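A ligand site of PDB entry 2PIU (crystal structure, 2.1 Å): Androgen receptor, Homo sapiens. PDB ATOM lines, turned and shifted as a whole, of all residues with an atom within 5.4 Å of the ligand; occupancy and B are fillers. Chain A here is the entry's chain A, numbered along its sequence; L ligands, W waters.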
ATOM      1  N   LEU A  33     -28.094   6.792 -16.988  1.00  0.00           N
ATOM      2  CA  LEU A  33     -29.113   7.764 -16.607  1.00  0.00           C
ATOM      3  C   LEU A  33     -29.538   7.633 -15.151  1.00  0.00           C
ATOM      4  O   LEU A  33     -29.825   8.632 -14.483  1.00  0.00           O
ATOM      5  CB  LEU A  33     -30.322   7.665 -17.540  1.00  0.00           C
ATOM      6  CG  LEU A  33     -30.195   8.490 -18.830  1.00  0.00           C
ATOM      7  CD1 LEU A  33     -30.105   9.982 -18.478  1.00  0.00           C
ATOM      8  CD2 LEU A  33     -28.949   8.056 -19.631  1.00  0.00           C
ATOM      9  N   LEU A  36     -26.994   9.428 -13.392  1.00  0.00           N
ATOM     10  CA  LEU A  36     -27.135  10.854 -13.633  1.00  0.00           C
ATOM     11  C   LEU A  36     -28.231  11.387 -12.727  1.00  0.00           C
ATOM     12  O   LEU A  36     -28.118  12.476 -12.173  1.00  0.00           O
ATOM     13  CB  LEU A  36     -27.496  11.123 -15.103  1.00  0.00           C
ATOM     14  CG  LEU A  36     -26.310  11.244 -16.060  1.00  0.00           C
ATOM     15  CD1 LEU A  36     -26.796  11.646 -17.444  1.00  0.00           C
ATOM     16  CD2 LEU A  36     -25.317  12.281 -15.538  1.00  0.00           C
ATOM     17  N   ASN A  37     -29.295  10.597 -12.554  1.00  0.00           N
ATOM     18  CA  ASN A  37     -30.414  10.998 -11.711  1.00  0.00           C
ATOM     19  C   ASN A  37     -30.042  11.009 -10.234  1.00  0.00           C
ATOM     20  O   ASN A  37     -30.471  11.896  -9.486  1.00  0.00           O
ATOM     21  CB  ASN A  37     -31.624  10.084 -11.927  1.00  0.00           C
ATOM     22  CG  ASN A  37     -32.330  10.355 -13.253  1.00  0.00           C
ATOM     23  OD1 ASN A  37     -32.235  11.459 -13.795  1.00  0.00           O
ATOM     24  ND2 ASN A  37     -33.049   9.367 -13.771  1.00  0.00           N
ATOM     25  N   LEU A  39     -27.121  11.495  -9.126  1.00  0.00           N
ATOM     26  CA  LEU A  39     -26.236  12.651  -9.003  1.00  0.00           C
ATOM     27  C   LEU A  39     -27.075  13.921  -8.932  1.00  0.00           C
ATOM     28  O   LEU A  39     -26.707  14.874  -8.230  1.00  0.00           O
ATOM     29  CB  LEU A  39     -25.296  12.719 -10.204  1.00  0.00           C
ATOM     30  CG  LEU A  39     -24.400  13.962 -10.254  1.00  0.00           C
ATOM     31  CD1 LEU A  39     -23.491  14.015  -9.032  1.00  0.00           C
ATOM     32  CD2 LEU A  39     -23.566  13.923 -11.530  1.00  0.00           C
ATOM     33  N   GLY A  40     -28.175  13.942  -9.672  1.00  0.00           N
ATOM     34  CA  GLY A  40     -29.039  15.107  -9.668  1.00  0.00           C
ATOM     35  C   GLY A  40     -29.617  15.241  -8.285  1.00  0.00           C
ATOM     36  O   GLY A  40     -29.593  16.326  -7.693  1.00  0.00           O
ATOM     37  N   GLN A  43     -26.923  16.501  -5.954  1.00  0.00           N
ATOM     38  CA  GLN A  43     -26.589  17.894  -6.153  1.00  0.00           C
ATOM     39  C   GLN A  43     -27.728  18.797  -5.694  1.00  0.00           C
ATOM     40  O   GLN A  43     -27.488  19.948  -5.306  1.00  0.00           O
ATOM     41  CB  GLN A  43     -26.219  18.150  -7.624  1.00  0.00           C
ATOM     42  CG  GLN A  43     -24.757  17.838  -7.923  1.00  0.00           C
ATOM     43  CD  GLN A  43     -24.330  18.116  -9.353  1.00  0.00           C
ATOM     44  OE1 GLN A  43     -24.700  19.122  -9.950  1.00  0.00           O
ATOM     45  NE2 GLN A  43     -23.533  17.210  -9.913  1.00  0.00           N
ATOM     46  N   TRP A  73     -32.583  24.619 -10.994  1.00  0.00           N
ATOM     47  CA  TRP A  73     -31.523  23.653 -10.723  1.00  0.00           C
ATOM     48  C   TRP A  73     -30.824  23.099 -11.974  1.00  0.00           C
ATOM     49  O   TRP A  73     -29.609  22.904 -11.967  1.00  0.00           O
ATOM     50  CB  TRP A  73     -32.044  22.489  -9.884  1.00  0.00           C
ATOM     51  CG  TRP A  73     -33.182  21.762 -10.509  1.00  0.00           C
ATOM     52  CD1 TRP A  73     -34.508  22.100 -10.458  1.00  0.00           C
ATOM     53  CD2 TRP A  73     -33.100  20.567 -11.299  1.00  0.00           C
ATOM     54  NE1 TRP A  73     -35.261  21.194 -11.177  1.00  0.00           N
ATOM     55  CE2 TRP A  73     -34.419  20.252 -11.701  1.00  0.00           C
ATOM     56  CE3 TRP A  73     -32.044  19.755 -11.713  1.00  0.00           C
ATOM     57  CZ2 TRP A  73     -34.709  19.134 -12.497  1.00  0.00           C
ATOM     58  CZ3 TRP A  73     -32.327  18.639 -12.502  1.00  0.00           C
ATOM     59  CH2 TRP A  73     -33.661  18.342 -12.881  1.00  0.00           C
ATOM     60  N   MET A  74     -31.576  22.852 -13.044  1.00  0.00           N
ATOM     61  CA  MET A  74     -30.964  22.290 -14.243  1.00  0.00           C
ATOM     62  C   MET A  74     -29.907  23.239 -14.803  1.00  0.00           C
ATOM     63  O   MET A  74     -28.772  22.819 -15.062  1.00  0.00           O
ATOM     64  CB  MET A  74     -32.029  21.987 -15.307  1.00  0.00           C
ATOM     65  CG  MET A  74     -31.480  21.323 -16.554  1.00  0.00           C
ATOM     66  SD  MET A  74     -31.059  19.572 -16.314  1.00  0.00           S
ATOM     67  CE  MET A  74     -32.693  18.839 -16.469  1.00  0.00           C
ATOM     68  N   MET A  77     -26.840  23.432 -12.339  1.00  0.00           N
ATOM     69  CA  MET A  77     -25.966  22.250 -12.404  1.00  0.00           C
ATOM     70  C   MET A  77     -25.232  22.104 -13.747  1.00  0.00           C
ATOM     71  O   MET A  77     -24.078  21.686 -13.780  1.00  0.00           O
ATOM     72  CB  MET A  77     -26.772  20.976 -12.116  1.00  0.00           C
ATOM     73  CG  MET A  77     -27.311  20.896 -10.690  1.00  0.00           C
ATOM     74  SD  MET A  77     -28.360  19.445 -10.397  1.00  0.00           S
ATOM     75  CE  MET A  77     -29.058  19.839  -8.766  1.00  0.00           C
ATOM     76  N   VAL A  78     -25.906  22.458 -14.832  1.00  0.00           N
ATOM     77  CA  VAL A  78     -25.285  22.373 -16.141  1.00  0.00           C
ATOM     78  C   VAL A  78     -24.100  23.333 -16.208  1.00  0.00           C
ATOM     79  O   VAL A  78     -23.016  22.985 -16.678  1.00  0.00           O
ATOM     80  CB  VAL A  78     -26.300  22.707 -17.257  1.00  0.00           C
ATOM     81  CG1 VAL A  78     -25.574  23.034 -18.557  1.00  0.00           C
ATOM     82  CG2 VAL A  78     -27.230  21.535 -17.473  1.00  0.00           C
ATOM     83  N   MET A  81     -21.266  22.209 -14.015  1.00  0.00           N
ATOM     84  CA  MET A  81     -20.630  21.076 -14.673  1.00  0.00           C
ATOM     85  C   MET A  81     -19.693  21.546 -15.782  1.00  0.00           C
ATOM     86  O   MET A  81     -18.538  21.121 -15.855  1.00  0.00           O
ATOM     87  CB  MET A  81     -21.701  20.140 -15.225  1.00  0.00           C
ATOM     88  CG  MET A  81     -21.174  18.823 -15.767  1.00  0.00           C
ATOM     89  SD  MET A  81     -20.679  18.918 -17.495  1.00  0.00           S
ATOM     90  CE  MET A  81     -22.308  18.912 -18.286  1.00  0.00           C
ATOM     91  N   ARG A  84     -16.621  22.716 -14.271  1.00  0.00           N
ATOM     92  CA  ARG A  84     -15.830  21.614 -13.749  1.00  0.00           C
ATOM     93  C   ARG A  84     -15.090  20.949 -14.895  1.00  0.00           C
ATOM     94  O   ARG A  84     -13.922  20.582 -14.788  1.00  0.00           O
ATOM     95  CB  ARG A  84     -16.719  20.556 -13.089  1.00  0.00           C
ATOM     96  CG  ARG A  84     -17.181  20.873 -11.694  1.00  0.00           C
ATOM     97  CD  ARG A  84     -17.590  19.580 -11.001  1.00  0.00           C
ATOM     98  NE  ARG A  84     -18.710  18.897 -11.664  1.00  0.00           N
ATOM     99  CZ  ARG A  84     -19.975  19.297 -11.595  1.00  0.00           C
ATOM    100  NH1 ARG A  84     -20.288  20.380 -10.892  1.00  0.00           N
ATOM    101  NH2 ARG A  84     -20.930  18.594 -12.185  1.00  0.00           N
ATOM    102  N   PHE A  96     -19.221  15.304 -15.056  1.00  0.00           N
ATOM    103  CA  PHE A  96     -20.400  15.334 -14.187  1.00  0.00           C
ATOM    104  C   PHE A  96     -19.960  15.157 -12.736  1.00  0.00           C
ATOM    105  O   PHE A  96     -20.362  15.908 -11.852  1.00  0.00           O
ATOM    106  CB  PHE A  96     -21.385  14.231 -14.583  1.00  0.00           C
ATOM    107  CG  PHE A  96     -22.056  14.452 -15.917  1.00  0.00           C
ATOM    108  CD1 PHE A  96     -22.928  15.528 -16.106  1.00  0.00           C
ATOM    109  CD2 PHE A  96     -21.819  13.602 -16.988  1.00  0.00           C
ATOM    110  CE1 PHE A  96     -23.541  15.739 -17.328  1.00  0.00           C
ATOM    111  CE2 PHE A  96     -22.428  13.810 -18.227  1.00  0.00           C
ATOM    112  CZ  PHE A  96     -23.292  14.883 -18.395  1.00  0.00           C
ATOM    113  N   MET A 112     -28.419  11.055 -25.445  1.00  0.00           N
ATOM    114  CA  MET A 112     -28.581  12.514 -25.443  1.00  0.00           C
ATOM    115  C   MET A 112     -27.276  13.115 -25.972  1.00  0.00           C
ATOM    116  O   MET A 112     -26.759  14.099 -25.449  1.00  0.00           O
ATOM    117  CB  MET A 112     -28.914  13.031 -24.025  1.00  0.00           C
ATOM    118  CG  MET A 112     -27.998  12.537 -22.913  1.00  0.00           C
ATOM    119  SD  MET A 112     -28.461  13.149 -21.247  1.00  0.00           S
ATOM    120  CE  MET A 112     -27.348  14.501 -21.051  1.00  0.00           C
ATOM    121  N   MET A 119     -23.533  20.920 -24.370  1.00  0.00           N
ATOM    122  CA  MET A 119     -22.923  21.097 -23.053  1.00  0.00           C
ATOM    123  C   MET A 119     -21.409  21.241 -23.117  1.00  0.00           C
ATOM    124  O   MET A 119     -20.831  22.015 -22.353  1.00  0.00           O
ATOM    125  CB  MET A 119     -23.307  19.937 -22.122  1.00  0.00           C
ATOM    126  CG  MET A 119     -24.786  19.992 -21.721  1.00  0.00           C
ATOM    127  SD  MET A 119     -25.177  18.960 -20.307  1.00  0.00           S
ATOM    128  CE  MET A 119     -25.694  17.440 -21.125  1.00  0.00           C
ATOM    129  N   LEU A 205     -32.711  19.690 -21.891  1.00  0.00           N
ATOM    130  CA  LEU A 205     -32.559  18.640 -20.877  1.00  0.00           C
ATOM    131  C   LEU A 205     -33.871  18.484 -20.126  1.00  0.00           C
ATOM    132  O   LEU A 205     -34.208  17.391 -19.668  1.00  0.00           O
ATOM    133  CB  LEU A 205     -31.406  18.986 -19.912  1.00  0.00           C
ATOM    134  CG  LEU A 205     -30.015  18.992 -20.585  1.00  0.00           C
ATOM    135  CD1 LEU A 205     -28.949  19.495 -19.612  1.00  0.00           C
ATOM    136  CD2 LEU A 205     -29.674  17.600 -21.082  1.00  0.00           C
ATOM    137  N   PHE A 208     -35.954  16.308 -22.308  1.00  0.00           N
ATOM    138  CA  PHE A 208     -35.413  14.970 -22.236  1.00  0.00           C
ATOM    139  C   PHE A 208     -35.736  14.222 -20.935  1.00  0.00           C
ATOM    140  O   PHE A 208     -36.246  13.096 -20.965  1.00  0.00           O
ATOM    141  CB  PHE A 208     -33.891  15.026 -22.440  1.00  0.00           C
ATOM    142  CG  PHE A 208     -33.265  13.685 -22.660  1.00  0.00           C
ATOM    143  CD1 PHE A 208     -32.827  12.925 -21.574  1.00  0.00           C
ATOM    144  CD2 PHE A 208     -33.167  13.157 -23.935  1.00  0.00           C
ATOM    145  CE1 PHE A 208     -32.298  11.650 -21.774  1.00  0.00           C
ATOM    146  CE2 PHE A 208     -32.639  11.873 -24.146  1.00  0.00           C
ATOM    147  CZ  PHE A 208     -32.206  11.121 -23.057  1.00  0.00           C
ATOM    148  N   THR A 209     -35.437  14.836 -19.799  1.00  0.00           N
ATOM    149  CA  THR A 209     -35.712  14.154 -18.538  1.00  0.00           C
ATOM    150  C   THR A 209     -37.210  13.942 -18.327  1.00  0.00           C
ATOM    151  O   THR A 209     -37.624  12.895 -17.836  1.00  0.00           O
ATOM    152  CB  THR A 209     -35.092  14.923 -17.324  1.00  0.00           C
ATOM    153  OG1 THR A 209     -35.151  14.087 -16.161  1.00  0.00           O
ATOM    154  CG2 THR A 209     -35.834  16.221 -17.048  1.00  0.00           C
ATOM    155  N   LEU A 212     -38.247  11.149 -20.249  1.00  0.00           N
ATOM    156  CA  LEU A 212     -37.600   9.982 -19.667  1.00  0.00           C
ATOM    157  C   LEU A 212     -38.330   9.490 -18.415  1.00  0.00           C
ATOM    158  O   LEU A 212     -38.434   8.285 -18.184  1.00  0.00           O
ATOM    159  CB  LEU A 212     -36.150  10.295 -19.340  1.00  0.00           C
ATOM    160  CG  LEU A 212     -35.328   9.117 -18.805  1.00  0.00           C
ATOM    161  CD1 LEU A 212     -35.475   7.916 -19.739  1.00  0.00           C
ATOM    162  CD2 LEU A 212     -33.873   9.515 -18.659  1.00  0.00           C
ATOM    163  N   PHE A 223     -35.497   7.006 -10.838  1.00  0.00           N
ATOM    164  CA  PHE A 223     -35.546   8.436 -10.540  1.00  0.00           C
ATOM    165  C   PHE A 223     -35.723   8.578  -9.030  1.00  0.00           C
ATOM    166  O   PHE A 223     -36.713   8.102  -8.481  1.00  0.00           O
ATOM    167  CB  PHE A 223     -36.730   9.132 -11.220  1.00  0.00           C
ATOM    168  CG  PHE A 223     -36.485   9.519 -12.658  1.00  0.00           C
ATOM    169  CD1 PHE A 223     -36.566   8.572 -13.670  1.00  0.00           C
ATOM    170  CD2 PHE A 223     -36.189  10.832 -12.997  1.00  0.00           C
ATOM    171  CE1 PHE A 223     -36.368   8.946 -15.009  1.00  0.00           C
ATOM    172  CE2 PHE A 223     -35.984  11.207 -14.329  1.00  0.00           C
ATOM    173  CZ  PHE A 223     -36.076  10.247 -15.330  1.00  0.00           C
ATOM    174  N   MET A 227     -36.185  14.159  -7.347  1.00  0.00           N
ATOM    175  CA  MET A 227     -36.107  14.363  -8.791  1.00  0.00           C
ATOM    176  C   MET A 227     -37.433  14.024  -9.468  1.00  0.00           C
ATOM    177  O   MET A 227     -37.921  14.771 -10.318  1.00  0.00           O
ATOM    178  CB  MET A 227     -34.983  13.509  -9.381  1.00  0.00           C
ATOM    179  CG  MET A 227     -33.571  13.956  -8.977  1.00  0.00           C
ATOM    180  SD  MET A 227     -32.948  15.359  -9.948  1.00  0.00           S
ATOM    181  CE  MET A 227     -33.898  16.672  -9.286  1.00  0.00           C
ATOM    182  N   ILE A 231     -39.688  16.866 -11.354  1.00  0.00           N
ATOM    183  CA  ILE A 231     -39.776  16.709 -12.787  1.00  0.00           C
ATOM    184  C   ILE A 231     -41.203  16.458 -13.268  1.00  0.00           C
ATOM    185  O   ILE A 231     -41.509  16.669 -14.440  1.00  0.00           O
ATOM    186  CB  ILE A 231     -38.812  15.579 -13.252  1.00  0.00           C
ATOM    187  CG1 ILE A 231     -37.372  16.007 -12.964  1.00  0.00           C
ATOM    188  CG2 ILE A 231     -39.003  15.277 -14.730  1.00  0.00           C
ATOM    189  CD1 ILE A 231     -36.365  14.911 -13.094  1.00  0.00           C
HETATM  190  C1  LIG L   1     -26.598  16.145 -12.936  1.00  0.00           C
HETATM  191  C2  LIG L   1     -25.668  17.173 -12.289  1.00  0.00           C
HETATM  192  C3  LIG L   1     -24.704  17.656 -13.411  1.00  0.00           C
HETATM  193  O1  LIG L   1     -23.519  17.630 -13.191  1.00  0.00           O
HETATM  194  C4  LIG L   1     -25.314  18.113 -14.707  1.00  0.00           C
HETATM  195  C5  LIG L   1     -26.251  17.021 -15.309  1.00  0.00           C
HETATM  196  C6  LIG L   1     -26.919  17.460 -16.659  1.00  0.00           C
HETATM  197  C7  LIG L   1     -27.804  16.328 -17.206  1.00  0.00           C
HETATM  198  C8  LIG L   1     -28.912  15.891 -16.180  1.00  0.00           C
HETATM  199  C9  LIG L   1     -28.233  15.464 -14.842  1.00  0.00           C
HETATM  200  C10 LIG L   1     -27.341  16.608 -14.223  1.00  0.00           C
HETATM  201  C11 LIG L   1     -29.362  14.986 -13.845  1.00  0.00           C
HETATM  202  C12 LIG L   1     -30.290  13.887 -14.360  1.00  0.00           C
HETATM  203  C13 LIG L   1     -30.892  14.208 -15.747  1.00  0.00           C
HETATM  204  C14 LIG L   1     -29.742  14.698 -16.711  1.00  0.00           C
HETATM  205  C15 LIG L   1     -30.505  14.898 -18.027  1.00  0.00           C
HETATM  206  C16 LIG L   1     -31.348  13.596 -18.081  1.00  0.00           C
HETATM  207  C17 LIG L   1     -31.381  13.060 -16.616  1.00  0.00           C
HETATM  208  O2  LIG L   1     -32.705  12.624 -16.304  1.00  0.00           O
HETATM  209  C18 LIG L   1     -32.020  15.296 -15.561  1.00  0.00           C
HETATM  210  C19 LIG L   1     -28.265  17.852 -13.856  1.00  0.00           C
HETATM  211  O   HOH W   1     -23.106  20.375 -11.570  1.00  0.00           O
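OD1 of Asn 37 lies within hydrogen-bond range of O2 of the ligand.
The side-chain hydroxyl (OG1) of Thr 209 sits at hydrogen-bond distance from an oxygen (O2) of the ligand, at 2.9 Å.
NH2 of Arg 84 is in hydrogen-bond range of O1 of the ligand (2.9 Å).
NE2 of Gln 43 lies close to O1 of the ligand (3.3 Å).
O of Leu 33 lies close to ND2 of Asn 37 (3.4 Å).
The guanidinium group (NH2) of Arg 84 is in hydrogen-bond range of the backbone carbonyl oxygen (O) of Phe 96 (2.8 Å).
OE1 of Gln 43 lies close to SD of Met 77.
Leu 33 touches the ligand.
Leu 36 touches the ligand (O to C11, 3.3 Å).
Leu 39 touches the ligand (CD2 to C2, 3.9 Å).
Met 74 touches the ligand.
Met 77 touches the ligand.
Met 81 touches the ligand (CG to O1, 3.7 Å).
Phe 96 touches the ligand.
Phe 208 touches the ligand (CD1 to C16, 3.9 Å).
Hydrophobic or aromatic side chains within 4 Å of the ligand: Leu 33, Leu 36, Leu 39, Met 74, Met 77, Met 81, Phe 96 and Phe 208.
Within 4 Å of the ligand: Leu 33, Leu 36, Asn 37, Leu 39, Gln 43, Met 74, Met 77, Met 81, Arg 84, Phe 96, Phe 208 and Thr 209.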
